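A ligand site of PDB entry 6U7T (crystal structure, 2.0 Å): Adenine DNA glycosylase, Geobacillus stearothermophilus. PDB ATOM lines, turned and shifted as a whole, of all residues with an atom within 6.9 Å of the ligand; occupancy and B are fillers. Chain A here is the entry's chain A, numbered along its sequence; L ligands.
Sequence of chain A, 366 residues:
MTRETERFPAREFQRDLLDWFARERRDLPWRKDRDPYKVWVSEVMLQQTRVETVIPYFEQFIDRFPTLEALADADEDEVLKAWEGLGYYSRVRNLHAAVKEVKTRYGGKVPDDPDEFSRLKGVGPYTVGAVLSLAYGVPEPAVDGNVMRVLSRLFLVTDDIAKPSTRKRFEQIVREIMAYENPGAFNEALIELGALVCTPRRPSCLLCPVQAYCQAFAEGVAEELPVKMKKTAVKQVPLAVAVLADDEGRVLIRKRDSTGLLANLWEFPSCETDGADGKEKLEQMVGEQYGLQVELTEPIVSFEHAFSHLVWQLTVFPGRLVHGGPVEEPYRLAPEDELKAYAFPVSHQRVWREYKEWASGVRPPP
SG of Cys 214 is bound to FE4 of the ligand (2.3 Å). An iron atom (FE2) of the ligand is bound by the side-chain sulfur (SG) of Cys 205 (2.3 Å). The side-chain sulfur of Cys 208 is bound to an iron atom (FE1) of the ligand (2.3 Å). The side-chain sulfur (SG) of Cys 198 is bound to an iron atom (FE3) of the ligand (2.3 Å).
The backbone carbonyl oxygen (O) of Val 197 lies within hydrogen-bond range of the backbone NH (N) of Ser 204. N of Val 210 lies close to SG of Cys 208. The side-chain sulfur of Cys 214 lies close to the backbone NH of Phe 217 (3.2 Å). SG of Cys 214 lies close to N of Ala 216. The backbone carbonyl oxygen (O) of Cys 198 lies within hydrogen-bond range of the guanidinium group (NH1) of Arg 153 (3.3 Å). O of Ala 222 sits at hydrogen-bond distance from NE of Arg 153 (3.0 Å). The backbone carbonyl oxygen (O) of Cys 198 is in hydrogen-bond range of the guanidinium group (NE) of Arg 149, at 2.8 Å. The backbone NH (N) of Cys 198 lies within hydrogen-bond range of the backbone carbonyl oxygen (O) of Leu 193 (2.9 Å).
Arg 153 touches the ligand (CD to S1, 3.8 Å). Val 197 touches the ligand. CB of Pro 203 touches S4 of the ligand, at 3.8 Å. Gln 211 touches the ligand (CA to S3, 3.4 Å). Ala 222 touches the ligand (CB to S1, 3.6 Å). Hydrophobic or aromatic side chains within 4 Å of the ligand: Val 197, Pro 203 and Ala 222. Nine residues have an atom within 4 Å of the ligand: Arg 153, Val 197, Cys 198, Pro 203, Cys 205, Cys 208, Gln 211, Cys 214 and Ala 222. The nearest printed residue that does not touch the ligand is Ser 204 (4.1 Å).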
ATOM      1  N   ARG A 149     -16.947  -5.162  31.741  1.00  0.00           N
ATOM      2  CA  ARG A 149     -17.720  -5.189  30.512  1.00  0.00           C
ATOM      3  C   ARG A 149     -18.276  -3.807  30.187  1.00  0.00           C
ATOM      4  O   ARG A 149     -18.282  -3.405  29.016  1.00  0.00           O
ATOM      5  CB  ARG A 149     -18.855  -6.198  30.623  1.00  0.00           C
ATOM      6  CG  ARG A 149     -19.690  -6.262  29.370  1.00  0.00           C
ATOM      7  CD  ARG A 149     -20.728  -7.362  29.415  1.00  0.00           C
ATOM      8  NE  ARG A 149     -21.658  -7.176  30.523  1.00  0.00           N
ATOM      9  CZ  ARG A 149     -21.561  -7.791  31.704  1.00  0.00           C
ATOM     10  NH1 ARG A 149     -20.589  -8.657  31.941  1.00  0.00           N
ATOM     11  NH2 ARG A 149     -22.466  -7.536  32.651  1.00  0.00           N
ATOM     12  N   VAL A 150     -18.765  -3.079  31.196  1.00  0.00           N
ATOM     13  CA  VAL A 150     -19.283  -1.727  30.976  1.00  0.00           C
ATOM     14  C   VAL A 150     -18.173  -0.808  30.500  1.00  0.00           C
ATOM     15  O   VAL A 150     -18.267  -0.165  29.451  1.00  0.00           O
ATOM     16  CB  VAL A 150     -19.917  -1.178  32.266  1.00  0.00           C
ATOM     17  CG1 VAL A 150     -20.331   0.263  32.068  1.00  0.00           C
ATOM     18  CG2 VAL A 150     -21.100  -2.019  32.683  1.00  0.00           C
ATOM     19  N   LEU A 151     -17.097  -0.735  31.291  1.00  0.00           N
ATOM     20  CA  LEU A 151     -16.028   0.209  31.024  1.00  0.00           C
ATOM     21  C   LEU A 151     -15.364  -0.070  29.681  1.00  0.00           C
ATOM     22  O   LEU A 151     -14.948   0.867  28.997  1.00  0.00           O
ATOM     23  CB  LEU A 151     -14.998   0.153  32.147  1.00  0.00           C
ATOM     24  CG  LEU A 151     -15.489   0.732  33.462  1.00  0.00           C
ATOM     25  CD1 LEU A 151     -14.376   0.640  34.484  1.00  0.00           C
ATOM     26  CD2 LEU A 151     -15.934   2.160  33.277  1.00  0.00           C
ATOM     27  N   ARG A 153     -16.892  -1.249  27.039  1.00  0.00           N
ATOM     28  CA  ARG A 153     -17.808  -0.759  26.012  1.00  0.00           C
ATOM     29  C   ARG A 153     -17.834   0.761  25.973  1.00  0.00           C
ATOM     30  O   ARG A 153     -17.818   1.361  24.889  1.00  0.00           O
ATOM     31  CB  ARG A 153     -19.214  -1.283  26.259  1.00  0.00           C
ATOM     32  CG  ARG A 153     -19.428  -2.627  25.670  1.00  0.00           C
ATOM     33  CD  ARG A 153     -20.482  -3.359  26.429  1.00  0.00           C
ATOM     34  NE  ARG A 153     -20.698  -4.672  25.852  1.00  0.00           N
ATOM     35  CZ  ARG A 153     -21.648  -5.511  26.241  1.00  0.00           C
ATOM     36  NH1 ARG A 153     -22.481  -5.168  27.204  1.00  0.00           N
ATOM     37  NH2 ARG A 153     -21.755  -6.683  25.637  1.00  0.00           N
ATOM     38  N   LEU A 154     -17.910   1.399  27.139  1.00  0.00           N
ATOM     39  CA  LEU A 154     -17.950   2.858  27.169  1.00  0.00           C
ATOM     40  C   LEU A 154     -16.722   3.439  26.483  1.00  0.00           C
ATOM     41  O   LEU A 154     -16.856   4.222  25.536  1.00  0.00           O
ATOM     42  CB  LEU A 154     -18.032   3.339  28.622  1.00  0.00           C
ATOM     43  CG  LEU A 154     -19.413   3.282  29.260  1.00  0.00           C
ATOM     44  CD1 LEU A 154     -19.304   3.814  30.672  1.00  0.00           C
ATOM     45  CD2 LEU A 154     -20.445   4.068  28.451  1.00  0.00           C
ATOM     46  N   LEU A 193     -25.636  -1.583  36.626  1.00  0.00           N
ATOM     47  CA  LEU A 193     -25.758  -1.284  35.202  1.00  0.00           C
ATOM     48  C   LEU A 193     -25.365  -2.476  34.366  1.00  0.00           C
ATOM     49  O   LEU A 193     -26.126  -2.911  33.490  1.00  0.00           O
ATOM     50  CB  LEU A 193     -24.900  -0.069  34.851  1.00  0.00           C
ATOM     51  CG  LEU A 193     -24.923   0.465  33.416  1.00  0.00           C
ATOM     52  CD1 LEU A 193     -26.303   0.899  32.956  1.00  0.00           C
ATOM     53  CD2 LEU A 193     -23.948   1.640  33.321  1.00  0.00           C
ATOM     54  N   VAL A 197     -28.633  -3.689  32.487  1.00  0.00           N
ATOM     55  CA  VAL A 197     -28.699  -3.047  31.182  1.00  0.00           C
ATOM     56  C   VAL A 197     -27.608  -3.557  30.252  1.00  0.00           C
ATOM     57  O   VAL A 197     -27.896  -4.285  29.286  1.00  0.00           O
ATOM     58  CB  VAL A 197     -28.606  -1.515  31.330  1.00  0.00           C
ATOM     59  CG1 VAL A 197     -28.704  -0.855  29.981  1.00  0.00           C
ATOM     60  CG2 VAL A 197     -29.695  -1.006  32.271  1.00  0.00           C
ATOM     61  N   CYS A 198     -26.371  -3.263  30.580  1.00  0.00           N
ATOM     62  CA  CYS A 198     -25.255  -3.523  29.678  1.00  0.00           C
ATOM     63  C   CYS A 198     -24.799  -4.972  29.820  1.00  0.00           C
ATOM     64  O   CYS A 198     -23.717  -5.273  30.312  1.00  0.00           O
ATOM     65  CB  CYS A 198     -24.108  -2.577  30.006  1.00  0.00           C
ATOM     66  SG  CYS A 198     -22.807  -2.665  28.746  1.00  0.00           S
ATOM     67  N   THR A 199     -25.636  -5.859  29.327  1.00  0.00           N
ATOM     68  CA  THR A 199     -25.461  -7.272  29.625  1.00  0.00           C
ATOM     69  C   THR A 199     -24.501  -7.937  28.653  1.00  0.00           C
ATOM     70  O   THR A 199     -24.261  -7.435  27.548  1.00  0.00           O
ATOM     71  CB  THR A 199     -26.807  -7.977  29.595  1.00  0.00           C
ATOM     72  OG1 THR A 199     -27.462  -7.722  28.344  1.00  0.00           O
ATOM     73  CG2 THR A 199     -27.692  -7.495  30.731  1.00  0.00           C
ATOM     74  N   PRO A 203     -27.055  -6.206  24.743  1.00  0.00           N
ATOM     75  CA  PRO A 203     -27.338  -5.194  25.770  1.00  0.00           C
ATOM     76  C   PRO A 203     -28.422  -4.229  25.299  1.00  0.00           C
ATOM     77  O   PRO A 203     -28.574  -3.970  24.109  1.00  0.00           O
ATOM     78  CB  PRO A 203     -26.000  -4.479  25.954  1.00  0.00           C
ATOM     79  CG  PRO A 203     -25.302  -4.664  24.652  1.00  0.00           C
ATOM     80  CD  PRO A 203     -25.743  -5.991  24.111  1.00  0.00           C
ATOM     81  N   SER A 204     -29.175  -3.699  26.260  1.00  0.00           N
ATOM     82  CA  SER A 204     -30.265  -2.767  25.959  1.00  0.00           C
ATOM     83  C   SER A 204     -29.708  -1.351  25.905  1.00  0.00           C
ATOM     84  O   SER A 204     -29.986  -0.500  26.753  1.00  0.00           O
ATOM     85  CB  SER A 204     -31.371  -2.890  27.004  1.00  0.00           C
ATOM     86  OG  SER A 204     -31.743  -4.246  27.200  1.00  0.00           O
ATOM     87  N   CYS A 205     -28.944  -1.083  24.847  1.00  0.00           N
ATOM     88  CA  CYS A 205     -28.274   0.208  24.754  1.00  0.00           C
ATOM     89  C   CYS A 205     -29.292   1.326  24.624  1.00  0.00           C
ATOM     90  O   CYS A 205     -29.106   2.421  25.165  1.00  0.00           O
ATOM     91  CB  CYS A 205     -27.285   0.205  23.566  1.00  0.00           C
ATOM     92  SG  CYS A 205     -26.086  -1.225  23.529  1.00  0.00           S
ATOM     93  N   LEU A 206     -30.412   1.065  23.951  1.00  0.00           N
ATOM     94  CA  LEU A 206     -31.447   2.095  23.839  1.00  0.00           C
ATOM     95  C   LEU A 206     -32.010   2.443  25.213  1.00  0.00           C
ATOM     96  O   LEU A 206     -32.074   3.625  25.586  1.00  0.00           O
ATOM     97  CB  LEU A 206     -32.563   1.624  22.904  1.00  0.00           C
ATOM     98  CG  LEU A 206     -32.135   1.253  21.484  1.00  0.00           C
ATOM     99  CD1 LEU A 206     -33.298   0.656  20.710  1.00  0.00           C
ATOM    100  CD2 LEU A 206     -31.556   2.453  20.753  1.00  0.00           C
ATOM    101  N   LEU A 207     -32.431   1.434  25.974  1.00  0.00           N
ATOM    102  CA  LEU A 207     -32.845   1.659  27.345  1.00  0.00           C
ATOM    103  C   LEU A 207     -31.716   2.252  28.183  1.00  0.00           C
ATOM    104  O   LEU A 207     -31.978   3.036  29.107  1.00  0.00           O
ATOM    105  CB  LEU A 207     -33.344   0.362  27.972  1.00  0.00           C
ATOM    106  CG  LEU A 207     -34.820  -0.007  27.831  1.00  0.00           C
ATOM    107  CD1 LEU A 207     -35.006  -1.505  28.028  1.00  0.00           C
ATOM    108  CD2 LEU A 207     -35.663   0.756  28.833  1.00  0.00           C
ATOM    109  N   CYS A 208     -30.449   1.908  27.864  1.00  0.00           N
ATOM    110  CA  CYS A 208     -29.327   2.318  28.705  1.00  0.00           C
ATOM    111  C   CYS A 208     -29.451   3.811  28.989  1.00  0.00           C
ATOM    112  O   CYS A 208     -29.899   4.567  28.129  1.00  0.00           O
ATOM    113  CB  CYS A 208     -27.971   1.971  28.053  1.00  0.00           C
ATOM    114  SG  CYS A 208     -26.505   2.470  29.018  1.00  0.00           S
ATOM    115  N   PRO A 209     -29.148   4.255  30.212  1.00  0.00           N
ATOM    116  CA  PRO A 209     -29.169   5.695  30.501  1.00  0.00           C
ATOM    117  C   PRO A 209     -27.965   6.452  29.987  1.00  0.00           C
ATOM    118  O   PRO A 209     -28.034   7.675  29.859  1.00  0.00           O
ATOM    119  CB  PRO A 209     -29.229   5.740  32.033  1.00  0.00           C
ATOM    120  CG  PRO A 209     -28.467   4.507  32.431  1.00  0.00           C
ATOM    121  CD  PRO A 209     -28.818   3.467  31.408  1.00  0.00           C
ATOM    122  N   VAL A 210     -26.859   5.763  29.702  1.00  0.00           N
ATOM    123  CA  VAL A 210     -25.643   6.444  29.244  1.00  0.00           C
ATOM    124  C   VAL A 210     -25.303   5.990  27.831  1.00  0.00           C
ATOM    125  O   VAL A 210     -24.121   5.859  27.471  1.00  0.00           O
ATOM    126  CB  VAL A 210     -24.484   6.200  30.232  1.00  0.00           C
ATOM    127  CG1 VAL A 210     -24.894   6.689  31.604  1.00  0.00           C
ATOM    128  CG2 VAL A 210     -24.104   4.727  30.302  1.00  0.00           C
ATOM    129  N   GLN A 211     -26.330   5.774  27.008  1.00  0.00           N
ATOM    130  CA  GLN A 211     -26.111   5.365  25.632  1.00  0.00           C
ATOM    131  C   GLN A 211     -25.442   6.456  24.814  1.00  0.00           C
ATOM    132  O   GLN A 211     -24.722   6.158  23.857  1.00  0.00           O
ATOM    133  CB  GLN A 211     -27.443   4.955  24.998  1.00  0.00           C
ATOM    134  CG  GLN A 211     -28.449   6.072  24.806  1.00  0.00           C
ATOM    135  CD  GLN A 211     -28.610   6.451  23.350  1.00  0.00           C
ATOM    136  OE1 GLN A 211     -28.888   5.596  22.508  1.00  0.00           O
ATOM    137  NE2 GLN A 211     -28.433   7.728  23.043  1.00  0.00           N
ATOM    138  N   ALA A 212     -25.654   7.731  25.169  1.00  0.00           N
ATOM    139  CA  ALA A 212     -25.002   8.823  24.464  1.00  0.00           C
ATOM    140  C   ALA A 212     -23.482   8.805  24.613  1.00  0.00           C
ATOM    141  O   ALA A 212     -22.769   9.274  23.721  1.00  0.00           O
ATOM    142  CB  ALA A 212     -25.563  10.160  24.964  1.00  0.00           C
ATOM    143  N   TYR A 213     -22.962   8.244  25.725  1.00  0.00           N
ATOM    144  CA  TYR A 213     -21.517   8.249  25.975  1.00  0.00           C
ATOM    145  C   TYR A 213     -20.803   7.003  25.470  1.00  0.00           C
ATOM    146  O   TYR A 213     -19.570   6.966  25.512  1.00  0.00           O
ATOM    147  CB  TYR A 213     -21.174   8.322  27.469  1.00  0.00           C
ATOM    148  CG  TYR A 213     -21.954   9.268  28.342  1.00  0.00           C
ATOM    149  CD1 TYR A 213     -23.330   9.148  28.492  1.00  0.00           C
ATOM    150  CD2 TYR A 213     -21.296  10.228  29.082  1.00  0.00           C
ATOM    151  CE1 TYR A 213     -24.023   9.995  29.319  1.00  0.00           C
ATOM    152  CE2 TYR A 213     -21.979  11.073  29.918  1.00  0.00           C
ATOM    153  CZ  TYR A 213     -23.349  10.952  30.037  1.00  0.00           C
ATOM    154  OH  TYR A 213     -24.029  11.806  30.873  1.00  0.00           O
ATOM    155  N   CYS A 214     -21.524   5.989  25.048  1.00  0.00           N
ATOM    156  CA  CYS A 214     -20.910   4.687  24.815  1.00  0.00           C
ATOM    157  C   CYS A 214     -20.351   4.647  23.395  1.00  0.00           C
ATOM    158  O   CYS A 214     -21.091   4.577  22.412  1.00  0.00           O
ATOM    159  CB  CYS A 214     -21.906   3.564  25.066  1.00  0.00           C
ATOM    160  SG  CYS A 214     -21.423   1.940  24.431  1.00  0.00           S
ATOM    161  N   GLN A 215     -19.015   4.682  23.316  1.00  0.00           N
ATOM    162  CA  GLN A 215     -18.357   4.701  22.008  1.00  0.00           C
ATOM    163  C   GLN A 215     -18.689   3.457  21.216  1.00  0.00           C
ATOM    164  O   GLN A 215     -18.864   3.528  19.990  1.00  0.00           O
ATOM    165  CB  GLN A 215     -16.852   4.878  22.208  1.00  0.00           C
ATOM    166  CG  GLN A 215     -16.533   6.124  23.052  1.00  0.00           C
ATOM    167  CD  GLN A 215     -15.055   6.295  23.366  1.00  0.00           C
ATOM    168  OE1 GLN A 215     -14.195   5.779  22.654  1.00  0.00           O
ATOM    169  NE2 GLN A 215     -14.761   7.040  24.432  1.00  0.00           N
ATOM    170  N   ALA A 216     -18.842   2.311  21.889  1.00  0.00           N
ATOM    171  CA  ALA A 216     -19.211   1.073  21.202  1.00  0.00           C
ATOM    172  C   ALA A 216     -20.563   1.189  20.523  1.00  0.00           C
ATOM    173  O   ALA A 216     -20.728   0.766  19.374  1.00  0.00           O
ATOM    174  CB  ALA A 216     -19.216  -0.100  22.188  1.00  0.00           C
ATOM    175  N   PHE A 217     -21.560   1.745  21.222  1.00  0.00           N
ATOM    176  CA  PHE A 217     -22.853   1.970  20.581  1.00  0.00           C
ATOM    177  C   PHE A 217     -22.698   2.871  19.363  1.00  0.00           C
ATOM    178  O   PHE A 217     -23.246   2.589  18.297  1.00  0.00           O
ATOM    179  CB  PHE A 217     -23.858   2.574  21.546  1.00  0.00           C
ATOM    180  CG  PHE A 217     -25.232   2.662  20.969  1.00  0.00           C
ATOM    181  CD1 PHE A 217     -25.828   1.531  20.426  1.00  0.00           C
ATOM    182  CD2 PHE A 217     -25.933   3.854  20.946  1.00  0.00           C
ATOM    183  CE1 PHE A 217     -27.082   1.593  19.873  1.00  0.00           C
ATOM    184  CE2 PHE A 217     -27.206   3.920  20.396  1.00  0.00           C
ATOM    185  CZ  PHE A 217     -27.781   2.784  19.860  1.00  0.00           C
ATOM    186  N   VAL A 221     -20.615  -1.848  17.963  1.00  0.00           N
ATOM    187  CA  VAL A 221     -19.774  -3.003  18.214  1.00  0.00           C
ATOM    188  C   VAL A 221     -19.865  -3.411  19.678  1.00  0.00           C
ATOM    189  O   VAL A 221     -18.997  -4.116  20.208  1.00  0.00           O
ATOM    190  CB  VAL A 221     -18.312  -2.712  17.819  1.00  0.00           C
ATOM    191  CG1 VAL A 221     -18.192  -2.535  16.310  1.00  0.00           C
ATOM    192  CG2 VAL A 221     -17.803  -1.475  18.549  1.00  0.00           C
ATOM    193  N   ALA A 222     -20.930  -2.962  20.351  1.00  0.00           N
ATOM    194  CA  ALA A 222     -21.164  -3.318  21.744  1.00  0.00           C
ATOM    195  C   ALA A 222     -21.137  -4.830  21.935  1.00  0.00           C
ATOM    196  O   ALA A 222     -20.538  -5.324  22.900  1.00  0.00           O
ATOM    197  CB  ALA A 222     -22.498  -2.758  22.222  1.00  0.00           C
ATOM    198  N   GLU A 223     -21.763  -5.580  21.019  1.00  0.00           N
ATOM    199  CA  GLU A 223     -21.808  -7.045  21.131  1.00  0.00           C
ATOM    200  C   GLU A 223     -20.468  -7.712  20.869  1.00  0.00           C
ATOM    201  O   GLU A 223     -20.337  -8.910  21.112  1.00  0.00           O
ATOM    202  CB  GLU A 223     -22.854  -7.602  20.163  1.00  0.00           C
ATOM    203  CG  GLU A 223     -24.196  -7.922  20.814  1.00  0.00           C
ATOM    204  CD  GLU A 223     -25.356  -7.842  19.838  1.00  0.00           C
ATOM    205  OE1 GLU A 223     -25.957  -6.751  19.717  1.00  0.00           O
ATOM    206  OE2 GLU A 223     -25.655  -8.860  19.183  1.00  0.00           O
HETATM  207 FE1  LIG L   1     -25.126   1.212  27.626  1.00  0.00          FE
HETATM  208 FE2  LIG L   1     -25.127   0.032  25.235  1.00  0.00          FE
HETATM  209 FE3  LIG L   1     -23.546  -1.009  27.357  1.00  0.00          FE
HETATM  210 FE4  LIG L   1     -22.836   1.245  26.173  1.00  0.00          FE
HETATM  211  S1  LIG L   1     -22.931  -0.750  25.167  1.00  0.00           S
HETATM  212  S2  LIG L   1     -23.005   0.840  28.383  1.00  0.00           S
HETATM  213  S3  LIG L   1     -24.865   2.167  25.631  1.00  0.00           S
HETATM  214  S4  LIG L   1     -25.877  -0.931  27.207  1.00  0.00           S
